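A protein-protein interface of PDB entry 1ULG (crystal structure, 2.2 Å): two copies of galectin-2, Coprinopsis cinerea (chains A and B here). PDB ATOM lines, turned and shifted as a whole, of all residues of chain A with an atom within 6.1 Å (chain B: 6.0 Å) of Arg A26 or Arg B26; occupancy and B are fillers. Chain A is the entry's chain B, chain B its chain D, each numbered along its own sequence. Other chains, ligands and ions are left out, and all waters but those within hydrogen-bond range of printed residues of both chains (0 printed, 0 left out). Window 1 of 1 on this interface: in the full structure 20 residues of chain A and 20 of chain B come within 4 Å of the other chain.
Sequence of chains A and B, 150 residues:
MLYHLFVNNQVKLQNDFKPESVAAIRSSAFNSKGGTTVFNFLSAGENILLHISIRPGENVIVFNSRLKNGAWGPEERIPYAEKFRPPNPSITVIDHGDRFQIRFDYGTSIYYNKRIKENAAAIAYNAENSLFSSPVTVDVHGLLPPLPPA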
ATOM      1  N   LEU A   2       9.048  16.376   3.064  1.00  0.00           N
ATOM      2  CA  LEU A   2      10.136  15.796   3.841  1.00  0.00           C
ATOM      3  C   LEU A   2       9.603  15.030   5.037  1.00  0.00           C
ATOM      4  O   LEU A   2       8.667  15.477   5.696  1.00  0.00           O
ATOM      5  CB  LEU A   2      11.084  16.888   4.361  1.00  0.00           C
ATOM      6  CG  LEU A   2      12.156  16.352   5.319  1.00  0.00           C
ATOM      7  CD1 LEU A   2      13.103  15.469   4.527  1.00  0.00           C
ATOM      8  CD2 LEU A   2      12.924  17.491   5.992  1.00  0.00           C
ATOM      9  N   HIS A   4      11.079  12.241   8.372  1.00  0.00           N
ATOM     10  CA  HIS A   4      12.216  11.671   9.076  1.00  0.00           C
ATOM     11  C   HIS A   4      11.741  10.285   9.472  1.00  0.00           C
ATOM     12  O   HIS A   4      10.898  10.118  10.356  1.00  0.00           O
ATOM     13  CB  HIS A   4      12.594  12.496  10.318  1.00  0.00           C
ATOM     14  CG  HIS A   4      13.327  13.764   9.996  1.00  0.00           C
ATOM     15  ND1 HIS A   4      12.765  15.014  10.155  1.00  0.00           N
ATOM     16  CD2 HIS A   4      14.564  13.971   9.483  1.00  0.00           C
ATOM     17  CE1 HIS A   4      13.623  15.934   9.753  1.00  0.00           C
ATOM     18  NE2 HIS A   4      14.723  15.327   9.339  1.00  0.00           N
ATOM     19  N   ALA A  24      13.306  10.076  -2.260  1.00  0.00           N
ATOM     20  CA  ALA A  24      14.753  10.163  -2.097  1.00  0.00           C
ATOM     21  C   ALA A  24      15.058   9.912  -0.625  1.00  0.00           C
ATOM     22  O   ALA A  24      14.731  10.729   0.228  1.00  0.00           O
ATOM     23  CB  ALA A  24      15.261  11.542  -2.530  1.00  0.00           C
ATOM     24  N   ILE A  25      15.661   8.762  -0.339  1.00  0.00           N
ATOM     25  CA  ILE A  25      16.014   8.366   1.022  1.00  0.00           C
ATOM     26  C   ILE A  25      17.501   8.589   1.248  1.00  0.00           C
ATOM     27  O   ILE A  25      18.323   8.018   0.532  1.00  0.00           O
ATOM     28  CB  ILE A  25      15.761   6.870   1.260  1.00  0.00           C
ATOM     29  CG1 ILE A  25      14.311   6.521   0.929  1.00  0.00           C
ATOM     30  CG2 ILE A  25      16.099   6.511   2.701  1.00  0.00           C
ATOM     31  CD1 ILE A  25      14.022   5.024   0.917  1.00  0.00           C
ATOM     32  N   ARG A  26      17.841   9.397   2.251  1.00  0.00           N
ATOM     33  CA  ARG A  26      19.235   9.673   2.565  1.00  0.00           C
ATOM     34  C   ARG A  26      19.580   9.500   4.050  1.00  0.00           C
ATOM     35  O   ARG A  26      18.804   9.868   4.941  1.00  0.00           O
ATOM     36  CB  ARG A  26      19.601  11.087   2.120  1.00  0.00           C
ATOM     37  CG  ARG A  26      19.360  11.347   0.643  1.00  0.00           C
ATOM     38  CD  ARG A  26      19.878  12.716   0.242  1.00  0.00           C
ATOM     39  NE  ARG A  26      19.187  13.797   0.943  1.00  0.00           N
ATOM     40  CZ  ARG A  26      19.811  14.835   1.493  1.00  0.00           C
ATOM     41  NH1 ARG A  26      21.134  14.916   1.422  1.00  0.00           N
ATOM     42  NH2 ARG A  26      19.116  15.798   2.093  1.00  0.00           N
ATOM     43  N   SER A  27      20.764   8.943   4.294  1.00  0.00           N
ATOM     44  CA  SER A  27      21.273   8.698   5.639  1.00  0.00           C
ATOM     45  C   SER A  27      22.457   9.626   5.959  1.00  0.00           C
ATOM     46  O   SER A  27      23.252   9.969   5.085  1.00  0.00           O
ATOM     47  CB  SER A  27      21.698   7.232   5.751  1.00  0.00           C
ATOM     48  OG  SER A  27      22.443   6.987   6.920  1.00  0.00           O
ATOM     49  N   SER A  28      22.567  10.036   7.215  1.00  0.00           N
ATOM     50  CA  SER A  28      23.657  10.923   7.626  1.00  0.00           C
ATOM     51  C   SER A  28      24.917  10.139   7.977  1.00  0.00           C
ATOM     52  O   SER A  28      26.006  10.710   8.052  1.00  0.00           O
ATOM     53  CB  SER A  28      23.227  11.770   8.826  1.00  0.00           C
ATOM     54  OG  SER A  28      22.509  10.989   9.768  1.00  0.00           O
ATOM     55  N   ASN A  88      27.165   9.487   3.525  1.00  0.00           N
ATOM     56  CA  ASN A  88      25.750   9.803   3.326  1.00  0.00           C
ATOM     57  C   ASN A  88      25.152   8.928   2.207  1.00  0.00           C
ATOM     58  O   ASN A  88      24.792   9.431   1.137  1.00  0.00           O
ATOM     59  CB  ASN A  88      25.581  11.285   2.948  1.00  0.00           C
ATOM     60  CG  ASN A  88      26.011  12.254   4.064  1.00  0.00           C
ATOM     61  OD1 ASN A  88      26.246  13.434   3.802  1.00  0.00           O
ATOM     62  ND2 ASN A  88      26.100  11.765   5.296  1.00  0.00           N
ATOM     63  N   PRO A  89      25.049   7.605   2.432  1.00  0.00           N
ATOM     64  CA  PRO A  89      24.479   6.764   1.369  1.00  0.00           C
ATOM     65  C   PRO A  89      23.003   7.077   1.107  1.00  0.00           C
ATOM     66  O   PRO A  89      22.293   7.539   1.996  1.00  0.00           O
ATOM     67  CB  PRO A  89      24.701   5.343   1.891  1.00  0.00           C
ATOM     68  CG  PRO A  89      24.647   5.521   3.394  1.00  0.00           C
ATOM     69  CD  PRO A  89      25.441   6.798   3.603  1.00  0.00           C
ATOM     70  N   SER A  90      22.547   6.819  -0.114  1.00  0.00           N
ATOM     71  CA  SER A  90      21.159   7.103  -0.472  1.00  0.00           C
ATOM     72  C   SER A  90      20.462   5.965  -1.205  1.00  0.00           C
ATOM     73  O   SER A  90      21.079   4.972  -1.595  1.00  0.00           O
ATOM     74  CB  SER A  90      21.087   8.346  -1.357  1.00  0.00           C
ATOM     75  OG  SER A  90      21.528   8.057  -2.678  1.00  0.00           O
ATOM     76  N   ILE A  91      19.163   6.143  -1.397  1.00  0.00           N
ATOM     77  CA  ILE A  91      18.332   5.177  -2.090  1.00  0.00           C
ATOM     78  C   ILE A  91      17.157   5.960  -2.650  1.00  0.00           C
ATOM     79  O   ILE A  91      16.403   6.601  -1.913  1.00  0.00           O
ATOM     80  CB  ILE A  91      17.804   4.080  -1.125  1.00  0.00           C
ATOM     81  CG1 ILE A  91      18.968   3.217  -0.625  1.00  0.00           C
ATOM     82  CG2 ILE A  91      16.760   3.235  -1.822  1.00  0.00           C
ATOM     83  CD1 ILE A  91      18.568   2.129   0.342  1.00  0.00           C
ATOM     84  N   SER A 133      21.622   5.743   9.355  1.00  0.00           N
ATOM     85  CA  SER A 133      21.249   6.572  10.492  1.00  0.00           C
ATOM     86  C   SER A 133      19.760   6.479  10.836  1.00  0.00           C
ATOM     87  O   SER A 133      18.925   6.108  10.003  1.00  0.00           O
ATOM     88  CB  SER A 133      21.590   8.033  10.202  1.00  0.00           C
ATOM     89  OG  SER A 133      20.830   8.525   9.107  1.00  0.00           O
ATOM     90  N   PRO A 135      16.884   8.977  12.432  1.00  0.00           N
ATOM     91  CA  PRO A 135      16.146   8.539  11.242  1.00  0.00           C
ATOM     92  C   PRO A 135      16.944   8.776   9.969  1.00  0.00           C
ATOM     93  O   PRO A 135      18.108   9.178  10.023  1.00  0.00           O
ATOM     94  CB  PRO A 135      14.922   9.433  11.278  1.00  0.00           C
ATOM     95  CG  PRO A 135      15.554  10.766  11.684  1.00  0.00           C
ATOM     96  CD  PRO A 135      16.488  10.350  12.815  1.00  0.00           C
ATOM     97  N   VAL A 136      16.320   8.498   8.825  1.00  0.00           N
ATOM     98  CA  VAL A 136      16.945   8.787   7.542  1.00  0.00           C
ATOM     99  C   VAL A 136      16.092   9.913   6.947  1.00  0.00           C
ATOM    100  O   VAL A 136      14.911  10.045   7.275  1.00  0.00           O
ATOM    101  CB  VAL A 136      16.942   7.585   6.549  1.00  0.00           C
ATOM    102  CG1 VAL A 136      18.057   6.620   6.893  1.00  0.00           C
ATOM    103  CG2 VAL A 136      15.581   6.896   6.548  1.00  0.00           C
ATOM    104  N   THR A 137      16.699  10.735   6.099  1.00  0.00           N
ATOM    105  CA  THR A 137      15.978  11.826   5.468  1.00  0.00           C
ATOM    106  C   THR A 137      15.255  11.271   4.245  1.00  0.00           C
ATOM    107  O   THR A 137      15.856  10.601   3.398  1.00  0.00           O
ATOM    108  CB  THR A 137      16.946  12.960   5.050  1.00  0.00           C
ATOM    109  OG1 THR A 137      17.297  13.722   6.209  1.00  0.00           O
ATOM    110  CG2 THR A 137      16.309  13.886   4.002  1.00  0.00           C
ATOM    111  N   VAL A 138      13.956  11.532   4.174  1.00  0.00           N
ATOM    112  CA  VAL A 138      13.158  11.070   3.050  1.00  0.00           C
ATOM    113  C   VAL A 138      12.393  12.218   2.407  1.00  0.00           C
ATOM    114  O   VAL A 138      11.572  12.868   3.053  1.00  0.00           O
ATOM    115  CB  VAL A 138      12.120  10.013   3.477  1.00  0.00           C
ATOM    116  CG1 VAL A 138      11.601   9.284   2.243  1.00  0.00           C
ATOM    117  CG2 VAL A 138      12.728   9.038   4.484  1.00  0.00           C
ATOM    118  N   ASP A 139      12.672  12.476   1.138  1.00  0.00           N
ATOM    119  CA  ASP A 139      11.953  13.514   0.405  1.00  0.00           C
ATOM    120  C   ASP A 139      11.107  12.805  -0.624  1.00  0.00           C
ATOM    121  O   ASP A 139      11.635  12.124  -1.495  1.00  0.00           O
ATOM    122  CB  ASP A 139      12.920  14.479  -0.275  1.00  0.00           C
ATOM    123  CG  ASP A 139      13.492  15.481   0.690  1.00  0.00           C
ATOM    124  OD1 ASP A 139      12.781  16.456   1.036  1.00  0.00           O
ATOM    125  OD2 ASP A 139      14.645  15.277   1.111  1.00  0.00           O
ATOM    126  N   LEU B   2      25.374  15.842   4.642  1.00  0.00           N
ATOM    127  CA  LEU B   2      24.103  15.758   5.361  1.00  0.00           C
ATOM    128  C   LEU B   2      24.264  15.377   6.824  1.00  0.00           C
ATOM    129  O   LEU B   2      24.974  14.429   7.159  1.00  0.00           O
ATOM    130  CB  LEU B   2      23.176  14.723   4.698  1.00  0.00           C
ATOM    131  CG  LEU B   2      21.994  14.245   5.558  1.00  0.00           C
ATOM    132  CD1 LEU B   2      20.968  15.364   5.708  1.00  0.00           C
ATOM    133  CD2 LEU B   2      21.344  13.010   4.926  1.00  0.00           C
ATOM    134  N   HIS B   4      22.024  15.056  10.749  1.00  0.00           N
ATOM    135  CA  HIS B   4      20.753  14.978  11.444  1.00  0.00           C
ATOM    136  C   HIS B   4      21.001  15.589  12.817  1.00  0.00           C
ATOM    137  O   HIS B   4      21.487  14.930  13.738  1.00  0.00           O
ATOM    138  CB  HIS B   4      20.300  13.526  11.549  1.00  0.00           C
ATOM    139  CG  HIS B   4      19.738  12.986  10.272  1.00  0.00           C
ATOM    140  ND1 HIS B   4      20.011  11.716   9.815  1.00  0.00           N
ATOM    141  CD2 HIS B   4      18.910  13.545   9.358  1.00  0.00           C
ATOM    142  CE1 HIS B   4      19.375  11.514   8.674  1.00  0.00           C
ATOM    143  NE2 HIS B   4      18.698  12.609   8.376  1.00  0.00           N
ATOM    144  N   ALA B  24      21.661  24.319   4.785  1.00  0.00           N
ATOM    145  CA  ALA B  24      20.220  24.286   4.528  1.00  0.00           C
ATOM    146  C   ALA B  24      19.548  23.392   5.565  1.00  0.00           C
ATOM    147  O   ALA B  24      19.641  22.167   5.489  1.00  0.00           O
ATOM    148  CB  ALA B  24      19.947  23.751   3.140  1.00  0.00           C
ATOM    149  N   ILE B  25      18.872  24.009   6.530  1.00  0.00           N
ATOM    150  CA  ILE B  25      18.202  23.263   7.590  1.00  0.00           C
ATOM    151  C   ILE B  25      16.718  23.120   7.281  1.00  0.00           C
ATOM    152  O   ILE B  25      16.041  24.103   6.974  1.00  0.00           O
ATOM    153  CB  ILE B  25      18.389  23.965   8.947  1.00  0.00           C
ATOM    154  CG1 ILE B  25      19.867  24.333   9.114  1.00  0.00           C
ATOM    155  CG2 ILE B  25      17.939  23.038  10.105  1.00  0.00           C
ATOM    156  CD1 ILE B  25      20.183  25.080  10.381  1.00  0.00           C
ATOM    157  N   ARG B  26      16.219  21.885   7.354  1.00  0.00           N
ATOM    158  CA  ARG B  26      14.818  21.616   7.055  1.00  0.00           C
ATOM    159  C   ARG B  26      14.181  20.753   8.139  1.00  0.00           C
ATOM    160  O   ARG B  26      14.822  19.870   8.714  1.00  0.00           O
ATOM    161  CB  ARG B  26      14.687  20.935   5.682  1.00  0.00           C
ATOM    162  CG  ARG B  26      15.090  21.815   4.499  1.00  0.00           C
ATOM    163  CD  ARG B  26      14.934  21.102   3.141  1.00  0.00           C
ATOM    164  NE  ARG B  26      15.784  19.918   3.027  1.00  0.00           N
ATOM    165  CZ  ARG B  26      15.355  18.724   2.618  1.00  0.00           C
ATOM    166  NH1 ARG B  26      14.084  18.558   2.276  1.00  0.00           N
ATOM    167  NH2 ARG B  26      16.186  17.686   2.584  1.00  0.00           N
ATOM    168  N   SER B  27      12.920  21.049   8.434  1.00  0.00           N
ATOM    169  CA  SER B  27      12.155  20.320   9.442  1.00  0.00           C
ATOM    170  C   SER B  27      11.008  19.567   8.777  1.00  0.00           C
ATOM    171  O   SER B  27      10.444  20.024   7.782  1.00  0.00           O
ATOM    172  CB  SER B  27      11.603  21.297  10.492  1.00  0.00           C
ATOM    173  OG  SER B  27      10.663  20.675  11.356  1.00  0.00           O
ATOM    174  N   SER B  28      10.676  18.406   9.330  1.00  0.00           N
ATOM    175  CA  SER B  28       9.593  17.583   8.800  1.00  0.00           C
ATOM    176  C   SER B  28       8.264  18.032   9.399  1.00  0.00           C
ATOM    177  O   SER B  28       7.206  17.495   9.078  1.00  0.00           O
ATOM    178  CB  SER B  28       9.849  16.115   9.137  1.00  0.00           C
ATOM    179  OG  SER B  28      10.235  15.981  10.493  1.00  0.00           O
ATOM    180  N   ASN B  88       6.853  21.878   6.280  1.00  0.00           N
ATOM    181  CA  ASN B  88       8.309  21.739   6.309  1.00  0.00           C
ATOM    182  C   ASN B  88       9.063  23.075   6.349  1.00  0.00           C
ATOM    183  O   ASN B  88       9.627  23.500   5.343  1.00  0.00           O
ATOM    184  CB  ASN B  88       8.794  20.966   5.084  1.00  0.00           C
ATOM    185  CG  ASN B  88       8.375  19.513   5.091  1.00  0.00           C
ATOM    186  OD1 ASN B  88       8.519  18.828   4.080  1.00  0.00           O
ATOM    187  ND2 ASN B  88       7.866  19.029   6.223  1.00  0.00           N
ATOM    188  N   PRO B  89       9.073  23.760   7.504  1.00  0.00           N
ATOM    189  CA  PRO B  89       9.790  25.038   7.588  1.00  0.00           C
ATOM    190  C   PRO B  89      11.305  24.875   7.419  1.00  0.00           C
ATOM    191  O   PRO B  89      11.878  23.849   7.800  1.00  0.00           O
ATOM    192  CB  PRO B  89       9.413  25.559   8.979  1.00  0.00           C
ATOM    193  CG  PRO B  89       9.090  24.316   9.746  1.00  0.00           C
ATOM    194  CD  PRO B  89       8.319  23.498   8.742  1.00  0.00           C
ATOM    195  N   SER B  90      11.952  25.883   6.846  1.00  0.00           N
ATOM    196  CA  SER B  90      13.398  25.816   6.649  1.00  0.00           C
ATOM    197  C   SER B  90      14.134  27.094   7.040  1.00  0.00           C
ATOM    198  O   SER B  90      13.550  28.180   7.126  1.00  0.00           O
ATOM    199  CB  SER B  90      13.727  25.499   5.185  1.00  0.00           C
ATOM    200  OG  SER B  90      13.501  26.637   4.363  1.00  0.00           O
ATOM    201  N   ILE B  91      15.433  26.931   7.267  1.00  0.00           N
ATOM    202  CA  ILE B  91      16.330  28.019   7.614  1.00  0.00           C
ATOM    203  C   ILE B  91      17.590  27.740   6.803  1.00  0.00           C
ATOM    204  O   ILE B  91      18.099  26.617   6.810  1.00  0.00           O
ATOM    205  CB  ILE B  91      16.691  28.023   9.112  1.00  0.00           C
ATOM    206  CG1 ILE B  91      15.422  28.028   9.959  1.00  0.00           C
ATOM    207  CG2 ILE B  91      17.519  29.257   9.436  1.00  0.00           C
ATOM    208  CD1 ILE B  91      15.677  28.065  11.452  1.00  0.00           C
ATOM    209  N   SER B 133      11.038  19.752  14.070  1.00  0.00           N
ATOM    210  CA  SER B 133      11.214  18.324  14.301  1.00  0.00           C
ATOM    211  C   SER B 133      12.577  18.003  14.894  1.00  0.00           C
ATOM    212  O   SER B 133      13.526  18.787  14.803  1.00  0.00           O
ATOM    213  CB  SER B 133      11.069  17.558  12.984  1.00  0.00           C
ATOM    214  OG  SER B 133      12.090  17.948  12.075  1.00  0.00           O
ATOM    215  N   PRO B 135      15.196  14.879  14.636  1.00  0.00           N
ATOM    216  CA  PRO B 135      16.096  15.977  14.284  1.00  0.00           C
ATOM    217  C   PRO B 135      15.584  16.789  13.109  1.00  0.00           C
ATOM    218  O   PRO B 135      14.484  16.570  12.597  1.00  0.00           O
ATOM    219  CB  PRO B 135      17.378  15.246  13.915  1.00  0.00           C
ATOM    220  CG  PRO B 135      16.837  14.072  13.151  1.00  0.00           C
ATOM    221  CD  PRO B 135      15.660  13.618  14.019  1.00  0.00           C
ATOM    222  N   VAL B 136      16.399  17.754  12.710  1.00  0.00           N
ATOM    223  CA  VAL B 136      16.114  18.573  11.548  1.00  0.00           C
ATOM    224  C   VAL B 136      17.172  18.062  10.580  1.00  0.00           C
ATOM    225  O   VAL B 136      18.214  17.566  11.008  1.00  0.00           O
ATOM    226  CB  VAL B 136      16.347  20.077  11.823  1.00  0.00           C
ATOM    227  CG1 VAL B 136      15.217  20.632  12.698  1.00  0.00           C
ATOM    228  CG2 VAL B 136      17.704  20.274  12.501  1.00  0.00           C
ATOM    229  N   THR B 137      16.892  18.146   9.290  1.00  0.00           N
ATOM    230  CA  THR B 137      17.841  17.705   8.281  1.00  0.00           C
ATOM    231  C   THR B 137      18.736  18.890   7.967  1.00  0.00           C
ATOM    232  O   THR B 137      18.245  20.010   7.803  1.00  0.00           O
ATOM    233  CB  THR B 137      17.105  17.238   6.995  1.00  0.00           C
ATOM    234  OG1 THR B 137      16.516  15.950   7.229  1.00  0.00           O
ATOM    235  CG2 THR B 137      18.061  17.155   5.804  1.00  0.00           C
ATOM    236  N   VAL B 138      20.045  18.660   7.907  1.00  0.00           N
ATOM    237  CA  VAL B 138      20.967  19.737   7.590  1.00  0.00           C
ATOM    238  C   VAL B 138      21.941  19.364   6.478  1.00  0.00           C
ATOM    239  O   VAL B 138      22.742  18.445   6.623  1.00  0.00           O
ATOM    240  CB  VAL B 138      21.792  20.170   8.821  1.00  0.00           C
ATOM    241  CG1 VAL B 138      22.559  21.468   8.500  1.00  0.00           C
ATOM    242  CG2 VAL B 138      20.883  20.355  10.037  1.00  0.00           C
ATOM    243  N   ASP B 139      21.850  20.062   5.354  1.00  0.00           N
ATOM    244  CA  ASP B 139      22.771  19.832   4.244  1.00  0.00           C
ATOM    245  C   ASP B 139      23.759  20.994   4.226  1.00  0.00           C
ATOM    246  O   ASP B 139      23.371  22.154   4.064  1.00  0.00           O
ATOM    247  CB  ASP B 139      22.017  19.744   2.915  1.00  0.00           C
ATOM    248  CG  ASP B 139      21.260  18.437   2.767  1.00  0.00           C
ATOM    249  OD1 ASP B 139      21.910  17.390   2.565  1.00  0.00           O
ATOM    250  OD2 ASP B 139      20.019  18.454   2.870  1.00  0.00           O
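Printed residues of chain B within 4 Å of Asn A88: Leu B2. Of the printed residues of chain B, Ser A133 touches His B4 (3.4 Å). Of the printed residues of chain B, Val A136 touches His B4 (3.8 Å). Of the printed residues of chain A, Leu B2 touches Arg A26, Ser A27, Ser A28 and Asn A88. Arg B26 touches just these residues of chain A: Leu A2, Arg A26 and Asp A139. Ser B90 touches none of the printed residues of chain A. The nearest printed residue of chain B that does not touch Arg A26 is Thr B137 (4.1 Å). The nearest residue of chain A that does not touch Arg B26 is Thr A137 (4.1 Å).
Hydrophobic or aromatic side chains of chain A that line the printed part of chain B: Leu A2, His A4 and Pro A135. Along chain A the printed residues that touch a printed residue of chain B span positions 2 to 139. Among the printed residues, 23 pairs touch across the chains. Among the printed residues, Asp or Glu carboxylates within 4 Å of a Lys or Arg side-chain nitrogen of the other chain: Arg A26 with Asp B139 (2.8 Å) and Asp A139 with Arg B26 (2.8 Å).
The backbone NH of Leu A2 lies within hydrogen-bond range of the side-chain amide oxygen of Asn B88. The side-chain hydroxyl (OG) of Ser B28 sits at hydrogen-bond distance from a ring nitrogen (ND1) of His A4 (2.7 Å). A ring nitrogen (ND1) of His A4 lies close to the backbone carbonyl oxygen of Pro B135 (3.4 Å). A ring nitrogen (NE2) of His A4 lies within hydrogen-bond range of the side-chain hydroxyl (OG1) of Thr B137 (2.8 Å). The guanidinium group (NH1) of Arg A26 is in salt-bridge range of the side-chain carboxylate (OD1) of Asp B139 (2.8 Å). The side-chain hydroxyl (OG) of Ser A28 lies within hydrogen-bond range of a ring nitrogen (ND1) of His B4, at 2.6 Å. The side-chain amide oxygen (OD1) of Asn A88 sits at hydrogen-bond distance from the backbone NH (N) of Leu B2 (2.7 Å). OG of Ser A133 sits close to ND1 of His B4, 3.4 Å away. O of Pro A135 sits close to ND1 of His B4 (3.2 Å). A ring nitrogen (NE2) of His B4 sits at hydrogen-bond distance from the side-chain hydroxyl of Thr A137, 2.8 Å away. OG1 of Thr A137 is in hydrogen-bond range of OG1 of Thr B137 (2.6 Å). The side-chain carboxylate (OD1) of Asp A139 is in salt-bridge range of the guanidinium group (NH1) of Arg B26 (2.8 Å).
Leu A2 touches Ser B28, and with the chains exchanged Ser A28 touches Leu B2. His A4 touches Thr B137, and with the chains exchanged Thr A137 touches His B4. Arg A26 touches its own counterpart, Arg B26. Arg A26 touches Asp B139, and with the chains exchanged Asp A139 touches Arg B26.
The backbone NH of Ser A27 lies within hydrogen-bond range of the backbone carbonyl oxygen of Pro A89 (3.1 Å). OG of Ser A27 sits at hydrogen-bond distance from N of Ser A133 (2.9 Å). The backbone carbonyl oxygen (O) of Pro A135 sits at hydrogen-bond distance from the side-chain hydroxyl (OG) of Ser A133, at 2.9 Å. N of Thr B137 sits at hydrogen-bond distance from O of Arg B26 (2.8 Å). O of Pro B89 sits at hydrogen-bond distance from N of Ser B27, at 3.1 Å. OG of Ser B133 sits at hydrogen-bond distance from O of Pro B135 (2.8 Å).
Among the printed residues, merely in contact across the chains: Leu A2 with Arg B26, Leu A2 with Ser B27, Leu A2 with Ser B28, His A4 with Ser B133, His A4 with Val B136, Arg A26 with Leu B2, Arg A26 with Arg B26, Ser A27 with Leu B2, Ser A28 with Leu B2, Pro A135 with Pro B135 and Val A136 with His B4.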
